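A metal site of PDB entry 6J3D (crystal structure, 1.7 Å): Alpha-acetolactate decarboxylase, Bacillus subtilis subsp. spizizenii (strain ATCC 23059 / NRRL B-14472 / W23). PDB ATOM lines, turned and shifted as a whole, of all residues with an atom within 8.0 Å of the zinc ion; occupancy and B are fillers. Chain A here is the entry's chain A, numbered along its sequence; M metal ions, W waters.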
ATOM      1  N   MET A  34      -3.454  35.881  18.225  1.00  0.00           N
ATOM      2  CA  MET A  34      -3.579  35.258  19.530  1.00  0.00           C
ATOM      3  C   MET A  34      -4.941  35.597  20.176  1.00  0.00           C
ATOM      4  O   MET A  34      -5.523  34.734  20.845  1.00  0.00           O
ATOM      5  CB  MET A  34      -2.369  35.680  20.434  1.00  0.00           C
ATOM      6  CG  MET A  34      -2.426  35.045  21.797  1.00  0.00           C
ATOM      7  SD  MET A  34      -2.236  33.242  21.692  1.00  0.00           S
ATOM      8  CE  MET A  34      -3.092  32.781  23.181  1.00  0.00           C
ATOM      9  N   LEU A  37      -7.518  33.129  19.046  1.00  0.00           N
ATOM     10  CA  LEU A  37      -7.367  31.873  19.735  1.00  0.00           C
ATOM     11  C   LEU A  37      -7.934  31.982  21.164  1.00  0.00           C
ATOM     12  O   LEU A  37      -8.618  31.081  21.646  1.00  0.00           O
ATOM     13  CB  LEU A  37      -5.886  31.426  19.723  1.00  0.00           C
ATOM     14  CG  LEU A  37      -5.639  29.960  19.901  1.00  0.00           C
ATOM     15  CD1 LEU A  37      -6.096  29.121  18.718  1.00  0.00           C
ATOM     16  CD2 LEU A  37      -4.140  29.799  20.113  1.00  0.00           C
ATOM     17  N   ILE A  59       6.347  27.505  15.264  1.00  0.00           N
ATOM     18  CA  ILE A  59       5.573  27.005  16.390  1.00  0.00           C
ATOM     19  C   ILE A  59       4.128  27.392  16.216  1.00  0.00           C
ATOM     20  O   ILE A  59       3.791  28.238  15.382  1.00  0.00           O
ATOM     21  CB  ILE A  59       6.068  27.608  17.737  1.00  0.00           C
ATOM     22  CG1 ILE A  59       5.930  29.136  17.773  1.00  0.00           C
ATOM     23  CG2 ILE A  59       7.523  27.093  18.066  1.00  0.00           C
ATOM     24  CD1 ILE A  59       6.176  29.709  19.148  1.00  0.00           C
ATOM     25  N   GLY A  60       3.269  26.741  16.989  1.00  0.00           N
ATOM     26  CA  GLY A  60       1.867  27.070  16.992  1.00  0.00           C
ATOM     27  C   GLY A  60       1.035  25.955  17.486  1.00  0.00           C
ATOM     28  O   GLY A  60       1.477  25.159  18.335  1.00  0.00           O
ATOM     29  N   THR A  61      -0.204  25.908  17.007  1.00  0.00           N
ATOM     30  CA  THR A  61      -1.065  24.779  17.349  1.00  0.00           C
ATOM     31  C   THR A  61      -1.814  24.289  16.101  1.00  0.00           C
ATOM     32  O   THR A  61      -1.472  24.671  14.984  1.00  0.00           O
ATOM     33  CB  THR A  61      -2.017  25.125  18.507  1.00  0.00           C
ATOM     34  OG1 THR A  61      -2.740  23.929  18.937  1.00  0.00           O
ATOM     35  CG2 THR A  61      -2.954  26.229  18.122  1.00  0.00           C
ATOM     36  N   GLU A  68       0.501  20.523  20.009  1.00  0.00           N
ATOM     37  CA  GLU A  68       1.415  21.643  19.854  1.00  0.00           C
ATOM     38  C   GLU A  68       2.231  21.454  18.589  1.00  0.00           C
ATOM     39  O   GLU A  68       2.742  20.379  18.348  1.00  0.00           O
ATOM     40  CB  GLU A  68       2.371  21.679  21.033  1.00  0.00           C
ATOM     41  CG  GLU A  68       1.705  21.785  22.415  1.00  0.00           C
ATOM     42  CD  GLU A  68       1.240  23.181  22.734  1.00  0.00           C
ATOM     43  OE1 GLU A  68       1.722  24.118  22.044  1.00  0.00           O
ATOM     44  OE2 GLU A  68       0.425  23.359  23.665  1.00  0.00           O
ATOM     45  N   LEU A  69       2.370  22.516  17.786  1.00  0.00           N
ATOM     46  CA  LEU A  69       3.226  22.512  16.599  1.00  0.00           C
ATOM     47  C   LEU A  69       4.644  22.987  16.930  1.00  0.00           C
ATOM     48  O   LEU A  69       4.817  23.979  17.644  1.00  0.00           O
ATOM     49  CB  LEU A  69       2.598  23.407  15.523  1.00  0.00           C
ATOM     50  CG  LEU A  69       3.374  23.642  14.233  1.00  0.00           C
ATOM     51  CD1 LEU A  69       3.473  22.414  13.353  1.00  0.00           C
ATOM     52  CD2 LEU A  69       2.731  24.775  13.430  1.00  0.00           C
ATOM     53  N   PHE A  96      -3.520  29.023  14.356  1.00  0.00           N
ATOM     54  CA  PHE A  96      -2.572  29.951  14.913  1.00  0.00           C
ATOM     55  C   PHE A  96      -1.192  29.355  14.855  1.00  0.00           C
ATOM     56  O   PHE A  96      -0.971  28.288  15.442  1.00  0.00           O
ATOM     57  CB  PHE A  96      -2.888  30.256  16.383  1.00  0.00           C
ATOM     58  CG  PHE A  96      -1.901  31.213  17.041  1.00  0.00           C
ATOM     59  CD1 PHE A  96      -1.945  32.565  16.741  1.00  0.00           C
ATOM     60  CD2 PHE A  96      -0.959  30.788  17.939  1.00  0.00           C
ATOM     61  CE1 PHE A  96      -1.073  33.490  17.306  1.00  0.00           C
ATOM     62  CE2 PHE A  96      -0.059  31.726  18.529  1.00  0.00           C
ATOM     63  CZ  PHE A  96      -0.127  33.067  18.182  1.00  0.00           C
ATOM     64  N   ARG A 148       3.506  22.428  28.606  1.00  0.00           N
ATOM     65  CA  ARG A 148       2.134  22.008  28.581  1.00  0.00           C
ATOM     66  C   ARG A 148       1.857  21.564  27.138  1.00  0.00           C
ATOM     67  O   ARG A 148       2.571  21.980  26.208  1.00  0.00           O
ATOM     68  CB  ARG A 148       1.247  23.181  28.956  1.00  0.00           C
ATOM     69  CG  ARG A 148       1.185  24.291  27.873  1.00  0.00           C
ATOM     70  CD  ARG A 148       0.039  24.176  26.825  1.00  0.00           C
ATOM     71  NE  ARG A 148       0.078  25.290  25.866  1.00  0.00           N
ATOM     72  CZ  ARG A 148      -0.307  26.536  26.128  1.00  0.00           C
ATOM     73  NH1 ARG A 148      -0.823  26.868  27.311  1.00  0.00           N
ATOM     74  NH2 ARG A 148      -0.186  27.467  25.191  1.00  0.00           N
ATOM     75  N   VAL A 150      -1.613  21.538  24.730  1.00  0.00           N
ATOM     76  CA  VAL A 150      -3.057  21.705  24.546  1.00  0.00           C
ATOM     77  C   VAL A 150      -3.635  20.432  23.933  1.00  0.00           C
ATOM     78  O   VAL A 150      -2.937  19.700  23.227  1.00  0.00           O
ATOM     79  CB  VAL A 150      -3.416  22.950  23.666  1.00  0.00           C
ATOM     80  CG1 VAL A 150      -3.024  24.267  24.403  1.00  0.00           C
ATOM     81  CG2 VAL A 150      -2.745  22.902  22.294  1.00  0.00           C
ATOM     82  N   MET A 160     -10.022  30.087  25.633  1.00  0.00           N
ATOM     83  CA  MET A 160      -8.763  29.390  25.913  1.00  0.00           C
ATOM     84  C   MET A 160      -8.368  29.458  27.378  1.00  0.00           C
ATOM     85  O   MET A 160      -7.752  28.512  27.867  1.00  0.00           O
ATOM     86  CB  MET A 160      -7.643  29.922  25.020  1.00  0.00           C
ATOM     87  CG  MET A 160      -6.454  28.926  24.882  1.00  0.00           C
ATOM     88  SD  MET A 160      -5.140  29.738  23.953  1.00  0.00           S
ATOM     89  CE  MET A 160      -3.865  28.462  24.176  1.00  0.00           C
ATOM     90  N   VAL A 180      12.616  26.086  20.441  1.00  0.00           N
ATOM     91  CA  VAL A 180      12.507  27.084  19.376  1.00  0.00           C
ATOM     92  C   VAL A 180      11.343  27.993  19.630  1.00  0.00           C
ATOM     93  O   VAL A 180      10.316  27.583  20.237  1.00  0.00           O
ATOM     94  CB  VAL A 180      12.371  26.497  17.947  1.00  0.00           C
ATOM     95  CG1 VAL A 180      13.696  25.831  17.521  1.00  0.00           C
ATOM     96  CG2 VAL A 180      11.165  25.569  17.830  1.00  0.00           C
ATOM     97  N   VAL A 193       2.273  36.570  20.709  1.00  0.00           N
ATOM     98  CA  VAL A 193       2.490  36.609  22.151  1.00  0.00           C
ATOM     99  C   VAL A 193       3.686  37.488  22.435  1.00  0.00           C
ATOM    100  O   VAL A 193       4.799  37.109  22.094  1.00  0.00           O
ATOM    101  CB  VAL A 193       2.742  35.168  22.697  1.00  0.00           C
ATOM    102  CG1 VAL A 193       3.087  35.179  24.233  1.00  0.00           C
ATOM    103  CG2 VAL A 193       1.550  34.224  22.331  1.00  0.00           C
ATOM    104  N   HIS A 197       8.085  33.358  23.336  1.00  0.00           N
ATOM    105  CA  HIS A 197       7.134  32.285  23.136  1.00  0.00           C
ATOM    106  C   HIS A 197       7.909  31.103  22.588  1.00  0.00           C
ATOM    107  O   HIS A 197       8.391  31.176  21.480  1.00  0.00           O
ATOM    108  CB  HIS A 197       6.044  32.696  22.141  1.00  0.00           C
ATOM    109  CG  HIS A 197       4.996  31.643  21.929  1.00  0.00           C
ATOM    110  ND1 HIS A 197       3.974  31.798  21.010  1.00  0.00           N
ATOM    111  CD2 HIS A 197       4.801  30.444  22.531  1.00  0.00           C
ATOM    112  CE1 HIS A 197       3.223  30.699  21.033  1.00  0.00           C
ATOM    113  NE2 HIS A 197       3.661  29.890  21.989  1.00  0.00           N
ATOM    114  N   LEU A 198       8.053  30.043  23.404  1.00  0.00           N
ATOM    115  CA  LEU A 198       8.969  28.950  23.114  1.00  0.00           C
ATOM    116  C   LEU A 198       8.270  27.599  23.229  1.00  0.00           C
ATOM    117  O   LEU A 198       7.432  27.401  24.118  1.00  0.00           O
ATOM    118  CB  LEU A 198      10.091  29.009  24.139  1.00  0.00           C
ATOM    119  CG  LEU A 198      10.827  30.323  24.292  1.00  0.00           C
ATOM    120  CD1 LEU A 198      11.858  30.250  25.461  1.00  0.00           C
ATOM    121  CD2 LEU A 198      11.531  30.689  22.981  1.00  0.00           C
ATOM    122  N   HIS A 199       8.591  26.699  22.288  1.00  0.00           N
ATOM    123  CA  HIS A 199       8.177  25.306  22.311  1.00  0.00           C
ATOM    124  C   HIS A 199       9.431  24.429  22.387  1.00  0.00           C
ATOM    125  O   HIS A 199      10.531  24.864  22.006  1.00  0.00           O
ATOM    126  CB  HIS A 199       7.380  24.980  21.059  1.00  0.00           C
ATOM    127  CG  HIS A 199       5.982  25.556  21.085  1.00  0.00           C
ATOM    128  ND1 HIS A 199       5.003  25.122  20.214  1.00  0.00           N
ATOM    129  CD2 HIS A 199       5.395  26.518  21.845  1.00  0.00           C
ATOM    130  CE1 HIS A 199       3.873  25.770  20.442  1.00  0.00           C
ATOM    131  NE2 HIS A 199       4.083  26.602  21.459  1.00  0.00           N
ATOM    132  N   GLY A 209       6.408  20.226  24.148  1.00  0.00           N
ATOM    133  CA  GLY A 209       5.211  21.041  24.105  1.00  0.00           C
ATOM    134  C   GLY A 209       5.547  22.507  24.229  1.00  0.00           C
ATOM    135  O   GLY A 209       6.653  22.911  23.906  1.00  0.00           O
ATOM    136  N   HIS A 210       4.588  23.292  24.688  1.00  0.00           N
ATOM    137  CA  HIS A 210       4.733  24.723  24.855  1.00  0.00           C
ATOM    138  C   HIS A 210       5.446  24.953  26.206  1.00  0.00           C
ATOM    139  O   HIS A 210       5.029  24.413  27.204  1.00  0.00           O
ATOM    140  CB  HIS A 210       3.358  25.365  24.868  1.00  0.00           C
ATOM    141  CG  HIS A 210       3.339  26.796  25.287  1.00  0.00           C
ATOM    142  ND1 HIS A 210       3.229  27.861  24.397  1.00  0.00           N
ATOM    143  CD2 HIS A 210       3.366  27.342  26.524  1.00  0.00           C
ATOM    144  CE1 HIS A 210       3.237  28.995  25.092  1.00  0.00           C
ATOM    145  NE2 HIS A 210       3.376  28.708  26.381  1.00  0.00           N
ATOM    146  N   VAL A 211       6.526  25.711  26.188  1.00  0.00           N
ATOM    147  CA  VAL A 211       7.384  25.899  27.348  1.00  0.00           C
ATOM    148  C   VAL A 211       6.865  26.915  28.340  1.00  0.00           C
ATOM    149  O   VAL A 211       6.531  28.063  27.967  1.00  0.00           O
ATOM    150  CB  VAL A 211       8.826  26.274  26.898  1.00  0.00           C
ATOM    151  CG1 VAL A 211       9.709  26.651  28.089  1.00  0.00           C
ATOM    152  CG2 VAL A 211       9.396  25.104  26.094  1.00  0.00           C
ATOM    153  N   PHE A 212       6.799  26.520  29.599  1.00  0.00           N
ATOM    154  CA  PHE A 212       6.525  27.454  30.726  1.00  0.00           C
ATOM    155  C   PHE A 212       7.739  27.856  31.524  1.00  0.00           C
ATOM    156  O   PHE A 212       7.839  28.989  32.067  1.00  0.00           O
ATOM    157  CB  PHE A 212       5.560  26.808  31.730  1.00  0.00           C
ATOM    158  CG  PHE A 212       4.121  26.799  31.299  1.00  0.00           C
ATOM    159  CD1 PHE A 212       3.619  27.733  30.378  1.00  0.00           C
ATOM    160  CD2 PHE A 212       3.249  25.865  31.852  1.00  0.00           C
ATOM    161  CE1 PHE A 212       2.261  27.718  30.003  1.00  0.00           C
ATOM    162  CE2 PHE A 212       1.919  25.841  31.482  1.00  0.00           C
ATOM    163  CZ  PHE A 212       1.417  26.774  30.547  1.00  0.00           C
ATOM    164  N   THR A 256      -2.643  32.095  29.690  1.00  0.00           N
ATOM    165  CA  THR A 256      -2.619  30.899  28.781  1.00  0.00           C
ATOM    166  C   THR A 256      -1.211  30.527  28.310  1.00  0.00           C
ATOM    167  O   THR A 256      -0.948  29.334  28.030  1.00  0.00           O
ATOM    168  CB  THR A 256      -3.536  31.081  27.552  1.00  0.00           C
ATOM    169  OG1 THR A 256      -3.064  32.135  26.728  1.00  0.00           O
ATOM    170  CG2 THR A 256      -4.950  31.406  27.991  1.00  0.00           C
ATOM    171  N   GLU A 257      -0.299  31.492  28.242  1.00  0.00           N
ATOM    172  CA  GLU A 257       1.048  31.246  27.692  1.00  0.00           C
ATOM    173  C   GLU A 257       2.184  31.267  28.689  1.00  0.00           C
ATOM    174  O   GLU A 257       3.217  30.651  28.440  1.00  0.00           O
ATOM    175  CB  GLU A 257       1.402  32.277  26.612  1.00  0.00           C
ATOM    176  CG  GLU A 257       0.290  32.466  25.602  1.00  0.00           C
ATOM    177  CD  GLU A 257       0.120  31.244  24.736  1.00  0.00           C
ATOM    178  OE1 GLU A 257       1.003  31.042  23.884  1.00  0.00           O
ATOM    179  OE2 GLU A 257      -0.895  30.507  24.910  1.00  0.00           O
HETATM  180 ZN    ZN M   1       2.753  27.997  22.332  1.00  0.00          ZN
HETATM  181  O   HOH W   1       1.345  28.078  20.476  1.00  0.00           O
HETATM  182  O   HOH W   2       1.138  26.653  22.395  1.00  0.00           O
HETATM  183  O   HOH W   3       0.769  28.925  22.594  1.00  0.00           O
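O of Glu 257 lies within hydrogen-bond range of NE2 of His 210 (2.8 Å). A ring nitrogen (ND1) of His 199 is in hydrogen-bond range of the backbone carbonyl oxygen of Leu 69 (2.8 Å). A ring nitrogen (NE2) of His 197 sits close to the side-chain carboxylate (OE1) of Glu 257 (3.5 Å). The backbone NH of His 199 is in hydrogen-bond range of the backbone carbonyl oxygen of Val 180. The side-chain hydroxyl (OG1) of Thr 256 is in hydrogen-bond range of the side-chain carboxylate (OE2) of Glu 257 (3.3 Å). The side-chain carboxylate of Glu 68 sits close to a ring nitrogen (NE2) of His 199 (3.5 Å). The side-chain carboxylate (OE2) of Glu 257 is in salt-bridge range of the guanidinium group (NH2) of Arg 148. The backbone NH (N) of His 210 sits at hydrogen-bond distance from the backbone carbonyl oxygen (O) of Arg 148.
Glu 257 touches the zinc ion. Of the 22 residues printed, 4 come within 4 Å of the zinc ion. Along chain A the residues within 4 Å of the zinc ion span positions 197 to 257. The nearest printed residue that does not touch the zinc ion is Glu 68 (4.02 Å).
Water W2 is bound to the zinc ion, 2.1 Å away. The zinc ion is bound by NE2 of His 199, at 2.1 Å. The zinc ion is bound by ND1 of His 210, 2.1 Å away. NE2 of His 197 is bound to the zinc ion (2.1 Å). Water W3 binds the zinc ion. The zinc ion is bound by water W1 (2.3 Å). The zinc ion has six donor atoms within binding distance.
Water W3 lies within hydrogen-bond range of OE1 of Glu 257 (2.5 Å) and NH2 of Arg 148 (3.1 Å). Water W2 lies within hydrogen-bond range of OE1 of Glu 68 (2.6 Å) and NH2 of Arg 148 (3.2 Å).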
